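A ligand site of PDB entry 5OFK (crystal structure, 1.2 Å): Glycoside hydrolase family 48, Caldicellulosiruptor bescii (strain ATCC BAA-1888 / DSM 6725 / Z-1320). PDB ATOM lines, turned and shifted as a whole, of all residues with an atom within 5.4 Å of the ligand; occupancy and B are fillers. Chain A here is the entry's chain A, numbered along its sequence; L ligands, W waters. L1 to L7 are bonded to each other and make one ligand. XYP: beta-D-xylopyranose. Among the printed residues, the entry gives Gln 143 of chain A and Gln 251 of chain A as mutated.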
ATOM      1  N   GLU A  49      18.423 -14.816   1.657  1.00  0.00           N
ATOM      2  CA  GLU A  49      19.371 -15.830   1.199  1.00  0.00           C
ATOM      3  C   GLU A  49      18.762 -17.228   1.218  1.00  0.00           C
ATOM      4  O   GLU A  49      19.041 -18.062   0.333  1.00  0.00           O
ATOM      5  CB  GLU A  49      20.626 -15.785   2.070  1.00  0.00           C
ATOM      6  CG  GLU A  49      21.748 -16.649   1.504  1.00  0.00           C
ATOM      7  CD  GLU A  49      23.060 -16.522   2.253  1.00  0.00           C
ATOM      8  OE1 GLU A  49      23.084 -15.854   3.324  1.00  0.00           O
ATOM      9  OE2 GLU A  49      24.062 -17.095   1.762  1.00  0.00           O
ATOM     10  N   ASN A  50      17.937 -17.511   2.232  1.00  0.00           N
ATOM     11  CA  ASN A  50      17.289 -18.821   2.359  1.00  0.00           C
ATOM     12  C   ASN A  50      15.849 -18.761   2.801  1.00  0.00           C
ATOM     13  O   ASN A  50      15.119 -19.741   2.594  1.00  0.00           O
ATOM     14  CB  ASN A  50      18.025 -19.713   3.362  1.00  0.00           C
ATOM     15  CG  ASN A  50      19.359 -20.136   2.863  1.00  0.00           C
ATOM     16  OD1 ASN A  50      19.474 -20.891   1.904  1.00  0.00           O
ATOM     17  ND2 ASN A  50      20.400 -19.611   3.493  1.00  0.00           N
ATOM     18  N   LYS A  53      12.745 -19.622   0.500  1.00  0.00           N
ATOM     19  CA  LYS A  53      12.762 -20.866  -0.231  1.00  0.00           C
ATOM     20  C   LYS A  53      11.672 -21.805   0.289  1.00  0.00           C
ATOM     21  O   LYS A  53      11.193 -21.666   1.419  1.00  0.00           O
ATOM     22  CB  LYS A  53      14.136 -21.527  -0.117  1.00  0.00           C
ATOM     23  CG  LYS A  53      15.199 -20.736  -0.831  1.00  0.00           C
ATOM     24  CD  LYS A  53      16.589 -21.236  -0.489  1.00  0.00           C
ATOM     25  CE  LYS A  53      17.612 -20.430  -1.259  1.00  0.00           C
ATOM     26  NZ  LYS A  53      19.032 -20.755  -0.938  1.00  0.00           N
ATOM     27  N   GLU A  55      11.569 -24.894   1.593  1.00  0.00           N
ATOM     28  CA  GLU A  55      11.736 -25.537   2.889  1.00  0.00           C
ATOM     29  C   GLU A  55      11.559 -24.559   4.030  1.00  0.00           C
ATOM     30  O   GLU A  55      11.224 -24.983   5.133  1.00  0.00           O
ATOM     31  CB  GLU A  55      13.095 -26.234   2.982  1.00  0.00           C
ATOM     32  CG  GLU A  55      14.257 -25.257   3.042  1.00  0.00           C
ATOM     33  CD  GLU A  55      15.633 -25.919   3.119  1.00  0.00           C
ATOM     34  OE1 GLU A  55      15.726 -27.147   2.916  1.00  0.00           O
ATOM     35  OE2 GLU A  55      16.620 -25.185   3.344  1.00  0.00           O
ATOM     36  N   HIS A  90      12.813 -15.159  -3.539  1.00  0.00           N
ATOM     37  CA  HIS A  90      13.626 -16.281  -4.003  1.00  0.00           C
ATOM     38  C   HIS A  90      13.323 -17.471  -3.105  1.00  0.00           C
ATOM     39  O   HIS A  90      13.618 -17.412  -1.907  1.00  0.00           O
ATOM     40  CB  HIS A  90      15.090 -15.856  -3.889  1.00  0.00           C
ATOM     41  CG  HIS A  90      16.067 -16.909  -4.309  1.00  0.00           C
ATOM     42  ND1 HIS A  90      16.359 -17.165  -5.630  1.00  0.00           N
ATOM     43  CD2 HIS A  90      16.830 -17.755  -3.579  1.00  0.00           C
ATOM     44  CE1 HIS A  90      17.263 -18.145  -5.698  1.00  0.00           C
ATOM     45  NE2 HIS A  90      17.546 -18.532  -4.466  1.00  0.00           N
ATOM     46  N   TRP A  94      11.981 -25.040  -7.070  1.00  0.00           N
ATOM     47  CA  TRP A  94      13.395 -25.392  -7.137  1.00  0.00           C
ATOM     48  C   TRP A  94      13.586 -26.821  -6.696  1.00  0.00           C
ATOM     49  O   TRP A  94      12.944 -27.254  -5.732  1.00  0.00           O
ATOM     50  CB  TRP A  94      14.214 -24.496  -6.221  1.00  0.00           C
ATOM     51  CG  TRP A  94      15.685 -24.554  -6.379  1.00  0.00           C
ATOM     52  CD1 TRP A  94      16.394 -24.981  -7.467  1.00  0.00           C
ATOM     53  CD2 TRP A  94      16.643 -24.099  -5.415  1.00  0.00           C
ATOM     54  NE1 TRP A  94      17.751 -24.826  -7.233  1.00  0.00           N
ATOM     55  CE2 TRP A  94      17.929 -24.284  -5.981  1.00  0.00           C
ATOM     56  CE3 TRP A  94      16.558 -23.556  -4.115  1.00  0.00           C
ATOM     57  CZ2 TRP A  94      19.094 -23.980  -5.299  1.00  0.00           C
ATOM     58  CZ3 TRP A  94      17.696 -23.253  -3.459  1.00  0.00           C
ATOM     59  CH2 TRP A  94      18.954 -23.448  -4.045  1.00  0.00           C
ATOM     60  N   GLN A  97      16.385 -27.471  -1.707  1.00  0.00           N
ATOM     61  CA  GLN A  97      15.790 -26.767  -0.562  1.00  0.00           C
ATOM     62  C   GLN A  97      14.273 -26.776  -0.640  1.00  0.00           C
ATOM     63  O   GLN A  97      13.595 -25.807  -0.294  1.00  0.00           O
ATOM     64  CB  GLN A  97      16.385 -25.372  -0.351  1.00  0.00           C
ATOM     65  CG  GLN A  97      17.818 -25.472   0.148  1.00  0.00           C
ATOM     66  CD  GLN A  97      18.479 -24.122   0.374  1.00  0.00           C
ATOM     67  OE1 GLN A  97      19.142 -23.592  -0.511  1.00  0.00           O
ATOM     68  NE2 GLN A  97      18.285 -23.566   1.547  1.00  0.00           N
ATOM     69  N   ASN A 142      13.723 -21.749 -10.459  1.00  0.00           N
ATOM     70  CA  ASN A 142      15.175 -21.710 -10.275  1.00  0.00           C
ATOM     71  C   ASN A 142      15.781 -23.003 -10.814  1.00  0.00           C
ATOM     72  O   ASN A 142      15.402 -24.120 -10.402  1.00  0.00           O
ATOM     73  CB  ASN A 142      15.455 -21.557  -8.772  1.00  0.00           C
ATOM     74  CG  ASN A 142      16.783 -20.901  -8.442  1.00  0.00           C
ATOM     75  OD1 ASN A 142      17.183 -19.946  -9.095  1.00  0.00           O
ATOM     76  ND2 ASN A 142      17.476 -21.418  -7.445  1.00  0.00           N
ATOM     77  N   GLN A 143      16.732 -22.873 -11.745  1.00  0.00           N
ATOM     78  CA  GLN A 143      17.646 -23.969 -12.115  1.00  0.00           C
ATOM     79  C   GLN A 143      16.914 -25.205 -12.656  1.00  0.00           C
ATOM     80  O   GLN A 143      17.226 -26.348 -12.290  1.00  0.00           O
ATOM     81  CB  GLN A 143      18.519 -24.333 -10.910  1.00  0.00           C
ATOM     82  CG  GLN A 143      19.365 -23.201 -10.397  1.00  0.00           C
ATOM     83  CD  GLN A 143      20.190 -23.598  -9.178  1.00  0.00           C
ATOM     84  OE1 GLN A 143      20.164 -24.757  -8.749  1.00  0.00           O
ATOM     85  NE2 GLN A 143      20.942 -22.645  -8.642  1.00  0.00           N
ATOM     86  N   ASN A 186      15.382 -18.088 -13.304  1.00  0.00           N
ATOM     87  CA  ASN A 186      16.694 -17.776 -12.731  1.00  0.00           C
ATOM     88  C   ASN A 186      17.621 -18.974 -12.869  1.00  0.00           C
ATOM     89  O   ASN A 186      17.215 -20.114 -12.606  1.00  0.00           O
ATOM     90  CB  ASN A 186      16.486 -17.403 -11.254  1.00  0.00           C
ATOM     91  CG  ASN A 186      17.693 -16.781 -10.611  1.00  0.00           C
ATOM     92  OD1 ASN A 186      18.344 -15.901 -11.189  1.00  0.00           O
ATOM     93  ND2 ASN A 186      18.006 -17.196  -9.399  1.00  0.00           N
ATOM     94  N   TYR A 188      22.120 -20.422 -13.220  1.00  0.00           N
ATOM     95  CA  TYR A 188      23.565 -20.280 -13.245  1.00  0.00           C
ATOM     96  C   TYR A 188      24.124 -20.954 -14.495  1.00  0.00           C
ATOM     97  O   TYR A 188      23.432 -21.698 -15.195  1.00  0.00           O
ATOM     98  CB  TYR A 188      24.244 -20.866 -11.991  1.00  0.00           C
ATOM     99  CG  TYR A 188      24.140 -22.363 -11.904  1.00  0.00           C
ATOM    100  CD1 TYR A 188      23.001 -22.954 -11.395  1.00  0.00           C
ATOM    101  CD2 TYR A 188      25.167 -23.181 -12.327  1.00  0.00           C
ATOM    102  CE1 TYR A 188      22.862 -24.313 -11.343  1.00  0.00           C
ATOM    103  CE2 TYR A 188      25.049 -24.556 -12.260  1.00  0.00           C
ATOM    104  CZ  TYR A 188      23.871 -25.119 -11.767  1.00  0.00           C
ATOM    105  OH  TYR A 188      23.692 -26.466 -11.670  1.00  0.00           O
ATOM    106  N   ASN A 189      25.416 -20.711 -14.759  1.00  0.00           N
ATOM    107  CA  ASN A 189      26.111 -21.310 -15.909  1.00  0.00           C
ATOM    108  C   ASN A 189      25.489 -20.856 -17.226  1.00  0.00           C
ATOM    109  O   ASN A 189      25.497 -21.587 -18.222  1.00  0.00           O
ATOM    110  CB  ASN A 189      26.222 -22.832 -15.825  1.00  0.00           C
ATOM    111  CG  ASN A 189      27.442 -23.309 -15.076  1.00  0.00           C
ATOM    112  OD1 ASN A 189      28.305 -22.529 -14.746  1.00  0.00           O
ATOM    113  ND2 ASN A 189      27.541 -24.604 -14.831  1.00  0.00           N
ATOM    114  N   ILE A 192      27.858 -21.141 -20.234  1.00  0.00           N
ATOM    115  CA  ILE A 192      28.075 -22.385 -20.966  1.00  0.00           C
ATOM    116  C   ILE A 192      27.122 -22.346 -22.150  1.00  0.00           C
ATOM    117  O   ILE A 192      25.907 -22.340 -21.969  1.00  0.00           O
ATOM    118  CB  ILE A 192      27.811 -23.614 -20.084  1.00  0.00           C
ATOM    119  CG1 ILE A 192      28.797 -23.646 -18.904  1.00  0.00           C
ATOM    120  CG2 ILE A 192      27.880 -24.897 -20.921  1.00  0.00           C
ATOM    121  CD1 ILE A 192      28.651 -24.848 -17.996  1.00  0.00           C
ATOM    122  N   GLN A 219      22.452 -15.741 -12.582  1.00  0.00           N
ATOM    123  CA  GLN A 219      22.990 -15.781 -11.218  1.00  0.00           C
ATOM    124  C   GLN A 219      24.369 -15.157 -11.146  1.00  0.00           C
ATOM    125  O   GLN A 219      24.689 -14.417 -10.205  1.00  0.00           O
ATOM    126  CB  GLN A 219      22.969 -17.209 -10.686  1.00  0.00           C
ATOM    127  CG  GLN A 219      21.538 -17.676 -10.403  1.00  0.00           C
ATOM    128  CD  GLN A 219      21.435 -19.026  -9.803  1.00  0.00           C
ATOM    129  OE1 GLN A 219      22.428 -19.650  -9.445  1.00  0.00           O
ATOM    130  NE2 GLN A 219      20.187 -19.492  -9.651  1.00  0.00           N
ATOM    131  N   HIS A 221      27.362 -16.579 -10.589  1.00  0.00           N
ATOM    132  CA  HIS A 221      28.270 -17.160  -9.597  1.00  0.00           C
ATOM    133  C   HIS A 221      29.534 -17.510 -10.361  1.00  0.00           C
ATOM    134  O   HIS A 221      29.610 -18.565 -10.997  1.00  0.00           O
ATOM    135  CB  HIS A 221      27.669 -18.416  -8.978  1.00  0.00           C
ATOM    136  CG  HIS A 221      26.567 -18.121  -8.031  1.00  0.00           C
ATOM    137  ND1 HIS A 221      26.755 -17.431  -6.862  1.00  0.00           N
ATOM    138  CD2 HIS A 221      25.248 -18.462  -8.066  1.00  0.00           C
ATOM    139  CE1 HIS A 221      25.601 -17.331  -6.220  1.00  0.00           C
ATOM    140  NE2 HIS A 221      24.682 -17.976  -6.920  1.00  0.00           N
ATOM    141  N   ILE A 222      30.499 -16.589 -10.366  1.00  0.00           N
ATOM    142  CA  ILE A 222      31.676 -16.651 -11.239  1.00  0.00           C
ATOM    143  C   ILE A 222      32.942 -16.663 -10.398  1.00  0.00           C
ATOM    144  O   ILE A 222      32.896 -16.800  -9.174  1.00  0.00           O
ATOM    145  CB  ILE A 222      31.650 -15.515 -12.276  1.00  0.00           C
ATOM    146  CG1 ILE A 222      31.771 -14.115 -11.630  1.00  0.00           C
ATOM    147  CG2 ILE A 222      30.368 -15.647 -13.119  1.00  0.00           C
ATOM    148  CD1 ILE A 222      31.862 -12.943 -12.610  1.00  0.00           C
ATOM    149  N   ASN A 223      34.091 -16.590 -11.072  1.00  0.00           N
ATOM    150  CA  ASN A 223      35.361 -16.564 -10.355  1.00  0.00           C
ATOM    151  C   ASN A 223      36.317 -15.658 -11.113  1.00  0.00           C
ATOM    152  O   ASN A 223      35.973 -15.130 -12.161  1.00  0.00           O
ATOM    153  CB  ASN A 223      35.918 -17.970 -10.054  1.00  0.00           C
ATOM    154  CG  ASN A 223      36.375 -18.720 -11.292  1.00  0.00           C
ATOM    155  OD1 ASN A 223      37.243 -18.258 -12.027  1.00  0.00           O
ATOM    156  ND2 ASN A 223      35.824 -19.903 -11.502  1.00  0.00           N
ATOM    157  N   TRP A 226      37.040 -17.209 -14.757  1.00  0.00           N
ATOM    158  CA  TRP A 226      36.040 -17.744 -15.668  1.00  0.00           C
ATOM    159  C   TRP A 226      34.670 -17.294 -15.172  1.00  0.00           C
ATOM    160  O   TRP A 226      34.463 -17.230 -13.962  1.00  0.00           O
ATOM    161  CB  TRP A 226      36.105 -19.278 -15.683  1.00  0.00           C
ATOM    162  CG  TRP A 226      35.245 -19.875 -16.755  1.00  0.00           C
ATOM    163  CD1 TRP A 226      35.629 -20.183 -18.029  1.00  0.00           C
ATOM    164  CD2 TRP A 226      33.852 -20.196 -16.664  1.00  0.00           C
ATOM    165  NE1 TRP A 226      34.559 -20.678 -18.728  1.00  0.00           N
ATOM    166  CE2 TRP A 226      33.453 -20.693 -17.922  1.00  0.00           C
ATOM    167  CE3 TRP A 226      32.917 -20.092 -15.649  1.00  0.00           C
ATOM    168  CZ2 TRP A 226      32.148 -21.113 -18.185  1.00  0.00           C
ATOM    169  CZ3 TRP A 226      31.606 -20.505 -15.901  1.00  0.00           C
ATOM    170  CH2 TRP A 226      31.235 -21.001 -17.171  1.00  0.00           C
ATOM    171  N   GLN A 251      22.731 -13.086  -8.405  1.00  0.00           N
ATOM    172  CA  GLN A 251      23.451 -13.733  -7.326  1.00  0.00           C
ATOM    173  C   GLN A 251      24.949 -13.574  -7.517  1.00  0.00           C
ATOM    174  O   GLN A 251      25.722 -14.507  -7.318  1.00  0.00           O
ATOM    175  CB  GLN A 251      23.074 -15.213  -7.208  1.00  0.00           C
ATOM    176  CG  GLN A 251      21.571 -15.409  -7.239  1.00  0.00           C
ATOM    177  CD  GLN A 251      21.082 -16.828  -7.030  1.00  0.00           C
ATOM    178  OE1 GLN A 251      19.873 -17.057  -7.077  1.00  0.00           O
ATOM    179  NE2 GLN A 251      21.936 -17.735  -6.778  1.00  0.00           N
ATOM    180  N   ASN A 258      40.034 -20.925  -8.960  1.00  0.00           N
ATOM    181  CA  ASN A 258      39.507 -21.677 -10.063  1.00  0.00           C
ATOM    182  C   ASN A 258      38.576 -22.766  -9.559  1.00  0.00           C
ATOM    183  O   ASN A 258      38.738 -23.300  -8.463  1.00  0.00           O
ATOM    184  CB  ASN A 258      40.643 -22.354 -10.836  1.00  0.00           C
ATOM    185  CG  ASN A 258      41.115 -21.553 -12.001  1.00  0.00           C
ATOM    186  OD1 ASN A 258      40.342 -21.192 -12.883  1.00  0.00           O
ATOM    187  ND2 ASN A 258      42.416 -21.279 -12.016  1.00  0.00           N
ATOM    188  N   TYR A 259      37.614 -23.103 -10.384  1.00  0.00           N
ATOM    189  CA  TYR A 259      36.637 -24.119 -10.032  1.00  0.00           C
ATOM    190  C   TYR A 259      37.287 -25.499  -9.966  1.00  0.00           C
ATOM    191  O   TYR A 259      37.969 -25.918 -10.901  1.00  0.00           O
ATOM    192  CB  TYR A 259      35.614 -24.116 -11.154  1.00  0.00           C
ATOM    193  CG  TYR A 259      34.523 -25.162 -11.050  1.00  0.00           C
ATOM    194  CD1 TYR A 259      33.616 -25.131 -10.013  1.00  0.00           C
ATOM    195  CD2 TYR A 259      34.386 -26.155 -12.013  1.00  0.00           C
ATOM    196  CE1 TYR A 259      32.595 -26.077  -9.946  1.00  0.00           C
ATOM    197  CE2 TYR A 259      33.377 -27.079 -11.965  1.00  0.00           C
ATOM    198  CZ  TYR A 259      32.496 -27.035 -10.921  1.00  0.00           C
ATOM    199  OH  TYR A 259      31.480 -27.977 -10.884  1.00  0.00           O
ATOM    200  N   TRP A 300      25.509 -11.811  -4.004  1.00  0.00           N
ATOM    201  CA  TRP A 300      25.075 -12.911  -3.138  1.00  0.00           C
ATOM    202  C   TRP A 300      25.847 -12.908  -1.813  1.00  0.00           C
ATOM    203  O   TRP A 300      26.541 -13.870  -1.455  1.00  0.00           O
ATOM    204  CB  TRP A 300      25.135 -14.263  -3.880  1.00  0.00           C
ATOM    205  CG  TRP A 300      24.166 -15.253  -3.325  1.00  0.00           C
ATOM    206  CD1 TRP A 300      24.465 -16.370  -2.612  1.00  0.00           C
ATOM    207  CD2 TRP A 300      22.730 -15.198  -3.400  1.00  0.00           C
ATOM    208  NE1 TRP A 300      23.303 -17.020  -2.231  1.00  0.00           N
ATOM    209  CE2 TRP A 300      22.229 -16.316  -2.719  1.00  0.00           C
ATOM    210  CE3 TRP A 300      21.822 -14.299  -3.984  1.00  0.00           C
ATOM    211  CZ2 TRP A 300      20.850 -16.571  -2.599  1.00  0.00           C
ATOM    212  CZ3 TRP A 300      20.472 -14.553  -3.875  1.00  0.00           C
ATOM    213  CH2 TRP A 300      19.990 -15.685  -3.193  1.00  0.00           C
ATOM    214  N   TRP A 308      28.299 -17.859   1.088  1.00  0.00           N
ATOM    215  CA  TRP A 308      27.968 -19.267   0.996  1.00  0.00           C
ATOM    216  C   TRP A 308      29.112 -20.085   0.430  1.00  0.00           C
ATOM    217  O   TRP A 308      29.126 -21.310   0.638  1.00  0.00           O
ATOM    218  CB  TRP A 308      26.732 -19.426   0.102  1.00  0.00           C
ATOM    219  CG  TRP A 308      27.006 -19.266  -1.358  1.00  0.00           C
ATOM    220  CD1 TRP A 308      27.392 -18.127  -2.008  1.00  0.00           C
ATOM    221  CD2 TRP A 308      26.917 -20.289  -2.358  1.00  0.00           C
ATOM    222  NE1 TRP A 308      27.574 -18.383  -3.349  1.00  0.00           N
ATOM    223  CE2 TRP A 308      27.279 -19.698  -3.587  1.00  0.00           C
ATOM    224  CE3 TRP A 308      26.595 -21.650  -2.323  1.00  0.00           C
ATOM    225  CZ2 TRP A 308      27.317 -20.438  -4.773  1.00  0.00           C
ATOM    226  CZ3 TRP A 308      26.647 -22.370  -3.514  1.00  0.00           C
ATOM    227  CH2 TRP A 308      26.986 -21.770  -4.714  1.00  0.00           C
ATOM    228  N   PHE A 312      30.207 -23.982   0.920  1.00  0.00           N
ATOM    229  CA  PHE A 312      30.025 -24.768  -0.303  1.00  0.00           C
ATOM    230  C   PHE A 312      31.290 -25.556  -0.637  1.00  0.00           C
ATOM    231  O   PHE A 312      31.222 -26.741  -1.002  1.00  0.00           O
ATOM    232  CB  PHE A 312      29.647 -23.843  -1.447  1.00  0.00           C
ATOM    233  CG  PHE A 312      29.283 -24.530  -2.750  1.00  0.00           C
ATOM    234  CD1 PHE A 312      28.238 -25.430  -2.801  1.00  0.00           C
ATOM    235  CD2 PHE A 312      29.928 -24.199  -3.924  1.00  0.00           C
ATOM    236  CE1 PHE A 312      27.868 -26.011  -4.019  1.00  0.00           C
ATOM    237  CE2 PHE A 312      29.557 -24.780  -5.141  1.00  0.00           C
ATOM    238  CZ  PHE A 312      28.537 -25.675  -5.180  1.00  0.00           C
HETATM  239  O1  XYP L   1      38.837 -23.084 -18.762  1.00  0.00           O
HETATM  240  C1  XYP L   1      37.827 -23.740 -18.163  1.00  0.00           C
HETATM  241  C2  XYP L   1      37.866 -23.453 -16.665  1.00  0.00           C
HETATM  242  C3  XYP L   1      36.763 -24.190 -16.006  1.00  0.00           C
HETATM  243  C4  XYP L   1      35.450 -23.818 -16.619  1.00  0.00           C
HETATM  244  C5  XYP L   1      35.419 -24.058 -18.136  1.00  0.00           C
HETATM  245  O2  XYP L   1      39.130 -23.862 -16.135  1.00  0.00           O
HETATM  246  O3  XYP L   1      36.726 -23.879 -14.593  1.00  0.00           O
HETATM  247  O4  XYP L   1      34.437 -24.643 -16.075  1.00  0.00           O
HETATM  248  O5  XYP L   1      36.520 -23.312 -18.764  1.00  0.00           O
HETATM  249  C1  XYP L   2      33.401 -23.991 -15.397  1.00  0.00           C
HETATM  250  C2  XYP L   2      32.312 -24.996 -15.085  1.00  0.00           C
HETATM  251  C3  XYP L   2      31.272 -24.385 -14.232  1.00  0.00           C
HETATM  252  C4  XYP L   2      31.845 -23.762 -13.006  1.00  0.00           C
HETATM  253  C5  XYP L   2      32.980 -22.841 -13.347  1.00  0.00           C
HETATM  254  O2  XYP L   2      31.763 -25.416 -16.346  1.00  0.00           O
HETATM  255  O3  XYP L   2      30.347 -25.413 -13.818  1.00  0.00           O
HETATM  256  O4  XYP L   2      30.863 -22.936 -12.383  1.00  0.00           O
HETATM  257  O5  XYP L   2      33.997 -23.565 -14.120  1.00  0.00           O
HETATM  258  C1  XYP L   3      30.308 -23.406 -11.169  1.00  0.00           C
HETATM  259  C2  XYP L   3      29.696 -22.256 -10.391  1.00  0.00           C
HETATM  260  C3  XYP L   3      28.901 -22.757  -9.228  1.00  0.00           C
HETATM  261  C4  XYP L   3      27.841 -23.711  -9.672  1.00  0.00           C
HETATM  262  C5  XYP L   3      28.488 -24.850 -10.446  1.00  0.00           C
HETATM  263  O2  XYP L   3      30.800 -21.468  -9.935  1.00  0.00           O
HETATM  264  O3  XYP L   3      28.301 -21.605  -8.591  1.00  0.00           O
HETATM  265  O4  XYP L   3      27.163 -24.291  -8.554  1.00  0.00           O
HETATM  266  O5  XYP L   3      29.182 -24.260 -11.601  1.00  0.00           O
HETATM  267  C1  XYP L   4      25.790 -23.920  -8.416  1.00  0.00           C
HETATM  268  C2  XYP L   4      25.278 -24.691  -7.229  1.00  0.00           C
HETATM  269  C3  XYP L   4      23.922 -24.180  -6.839  1.00  0.00           C
HETATM  270  C4  XYP L   4      23.929 -22.723  -6.544  1.00  0.00           C
HETATM  271  C5  XYP L   4      24.508 -22.006  -7.747  1.00  0.00           C
HETATM  272  O2  XYP L   4      25.180 -26.069  -7.600  1.00  0.00           O
HETATM  273  O3  XYP L   4      23.449 -24.907  -5.670  1.00  0.00           O
HETATM  274  O4  XYP L   4      22.598 -22.285  -6.241  1.00  0.00           O
HETATM  275  O5  XYP L   4      25.852 -22.519  -7.996  1.00  0.00           O
HETATM  276  C1  XYP L   5      22.321 -20.874  -6.231  1.00  0.00           C
HETATM  277  C2  XYP L   5      20.943 -20.705  -5.633  1.00  0.00           C
HETATM  278  C3  XYP L   5      20.972 -20.019  -4.316  1.00  0.00           C
HETATM  279  C4  XYP L   5      21.994 -20.670  -3.446  1.00  0.00           C
HETATM  280  C5  XYP L   5      23.403 -20.491  -4.024  1.00  0.00           C
HETATM  281  O2  XYP L   5      20.093 -20.036  -6.554  1.00  0.00           O
HETATM  282  O3  XYP L   5      19.686 -20.126  -3.644  1.00  0.00           O
HETATM  283  O4  XYP L   5      21.948 -20.122  -2.114  1.00  0.00           O
HETATM  284  O5  XYP L   5      23.386 -20.211  -5.461  1.00  0.00           O
HETATM  285  C1  XYP L   6      22.613 -20.887  -1.151  1.00  0.00           C
HETATM  286  C2  XYP L   6      22.703 -20.099   0.130  1.00  0.00           C
HETATM  287  C3  XYP L   6      23.222 -20.940   1.244  1.00  0.00           C
HETATM  288  C4  XYP L   6      22.439 -22.196   1.412  1.00  0.00           C
HETATM  289  C5  XYP L   6      22.374 -22.919   0.069  1.00  0.00           C
HETATM  290  O2  XYP L   6      23.545 -18.966  -0.158  1.00  0.00           O
HETATM  291  O3  XYP L   6      23.140 -20.138   2.444  1.00  0.00           O
HETATM  292  O4  XYP L   6      23.078 -23.074   2.344  1.00  0.00           O
HETATM  293  O5  XYP L   6      21.755 -22.054  -0.898  1.00  0.00           O
HETATM  294  C1  XYP L   7      22.201 -23.660   3.182  1.00  0.00           C
HETATM  295  C2  XYP L   7      22.954 -24.813   3.846  1.00  0.00           C
HETATM  296  C3  XYP L   7      22.119 -25.462   4.905  1.00  0.00           C
HETATM  297  C4  XYP L   7      21.563 -24.465   5.880  1.00  0.00           C
HETATM  298  C5  XYP L   7      20.855 -23.301   5.168  1.00  0.00           C
HETATM  299  O2  XYP L   7      23.314 -25.777   2.851  1.00  0.00           O
HETATM  300  O3  XYP L   7      22.944 -26.421   5.620  1.00  0.00           O
HETATM  301  O4  XYP L   7      20.625 -25.132   6.730  1.00  0.00           O
HETATM  302  O5  XYP L   7      21.748 -22.663   4.193  1.00  0.00           O
HETATM  303  O   HOH W   1      23.004 -27.219  -8.973  1.00  0.00           O
HETATM  304  O   HOH W   2      40.450 -21.368 -15.591  1.00  0.00           O
HETATM  305  O   HOH W   3      24.868 -27.858  -5.442  1.00  0.00           O
HETATM  306  O   HOH W   4      39.341 -19.873 -17.677  1.00  0.00           O
HETATM  307  O   HOH W   5      23.213 -20.748   5.853  1.00  0.00           O
HETATM  308  O   HOH W   6      21.298 -26.327  -6.700  1.00  0.00           O
HETATM  309  O   HOH W   7      31.157 -19.992 -12.633  1.00  0.00           O
HETATM  310  O   HOH W   8      39.321 -24.941 -13.233  1.00  0.00           O
HETATM  311  O   HOH W   9      18.977 -26.202   4.185  1.00  0.00           O
HETATM  312  O   HOH W  10      32.391 -25.679 -18.985  1.00  0.00           O
HETATM  313  O   HOH W  11      23.193 -24.261  -2.987  1.00  0.00           O
HETATM  314  O   HOH W  12      30.934 -20.488  -7.407  1.00  0.00           O
HETATM  315  O   HOH W  13      33.771 -21.217 -10.057  1.00  0.00           O
HETATM  316  O   HOH W  14      37.541 -21.841 -13.060  1.00  0.00           O
HETATM  317  O   HOH W  15      25.826 -24.907   1.087  1.00  0.00           O
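An oxygen (O2) of XYP L6 lies within hydrogen-bond range of the side-chain carboxylate of Glu 49 (2.7 Å).
A ring nitrogen (NE2) of His 90 lies within hydrogen-bond range of an oxygen (O3) of XYP L5, 2.8 Å away.
NE1 of Trp 300 is in hydrogen-bond range of O2 of XYP L6 (2.9 Å).
The side-chain amino group (NZ) of Lys 53 lies within hydrogen-bond range of an oxygen (O3) of XYP L5 (2.9 Å).
NE2 of Gln 143 is in hydrogen-bond range of O4 of XYP L4, at 2.9 Å.
The side-chain amide nitrogen of Gln 251 lies within hydrogen-bond range of an oxygen (O2) of XYP L5, 3.0 Å away.
O2 of XYP L3 lies within hydrogen-bond range of O of His 221 (3.3 Å).
NE2 of His 221 lies within hydrogen-bond range of O5 of XYP L5, 3.0 Å away.
The side-chain amide nitrogen of Asn 50 is in hydrogen-bond range of an oxygen (O3) of XYP L6 (3.0 Å).
OE1 of Gln 97 lies close to O5 of XYP L6, 3.1 Å away.
The side-chain amide nitrogen of Asn 142 is in hydrogen-bond range of an oxygen (O2) of XYP L5 (3.1 Å).
The side-chain amide nitrogen (ND2) of Asn 189 is in hydrogen-bond range of an oxygen (O3) of XYP L2.
An oxygen (O2) of XYP L5 lies within hydrogen-bond range of the side-chain amide nitrogen (NE2) of Gln 219 (3.1 Å).
O5 of XYP L1 is in hydrogen-bond range of NE1 of Trp 226 (3.3 Å).
The side-chain amino group (NZ) of Lys 53 is in hydrogen-bond range of the backbone carbonyl oxygen (O) of Glu 49, 3.0 Å away.
The side-chain amino group of Lys 53 sits at hydrogen-bond distance from the side-chain amide oxygen of Asn 50.
The side-chain amide nitrogen (NE2) of Gln 143 lies close to the side-chain amide nitrogen (NE2) of Gln 219 (3.4 Å).
NE2 of His 221 lies within hydrogen-bond range of NE2 of Gln 251 (2.8 Å).
The side-chain amide nitrogen (ND2) of Asn 186 is in hydrogen-bond range of the side-chain amide oxygen (OE1) of Gln 251 (3.0 Å).
The side-chain amide oxygen (OD1) of Asn 50 sits at hydrogen-bond distance from the side-chain amide nitrogen (NE2) of Gln 97 (2.9 Å).
O of Gln 97 lies within hydrogen-bond range of N of Glu 55, at 2.9 Å.
OD1 of Asn 142 is in hydrogen-bond range of ND2 of Asn 186.
Merely in contact with the ligand: Trp 308 (3.2 Å), Tyr 259 (3.4 Å), Trp 94 (3.4 Å), Ile 192 (3.6 Å), Tyr 188 (3.8 Å) and Phe 312 (3.9 Å).
Hydrophobic or aromatic side chains within 4 Å of the ligand: His 90, Trp 94, Tyr 188, Ile 192, His 221, Trp 226, Tyr 259, Trp 300, Trp 308 and Phe 312.
Within 4 Å of the ligand: Glu 49, Asn 50, Lys 53, His 90, Trp 94, Gln 97, Asn 142, Gln 143, Tyr 188, Asn 189, Ile 192, Gln 219, His 221, Trp 226, Gln 251, Tyr 259, Trp 300, Trp 308 and Phe 312.
The nearest printed residue that does not touch the ligand is Asn 258 (4.4 Å).
Water W14 lies within hydrogen-bond range of O3 of XYP L1, OD1 of Asn 258, N of Tyr 259 and ND2 of Asn 223.
Water W6 bridges an oxygen (O3) of XYP L4 (2.8 Å) and the side-chain amide oxygen of Gln 143 (2.8 Å).
Water W2 bridges the side-chain amide oxygen (OD1) of Asn 258 (2.7 Å) and an oxygen (O2) of XYP L1 (2.9 Å).
Water W7 lies within hydrogen-bond range of the backbone carbonyl oxygen of His 221 (2.7 Å) and an oxygen (O4) of XYP L2 (3.0 Å).
Water W8 bridges O of Tyr 259 (2.9 Å) and O2 of XYP L1 (3.1 Å).
Water W9 bridges OE2 of Glu 55 (2.7 Å) and O4 of XYP L7 (3.2 Å).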
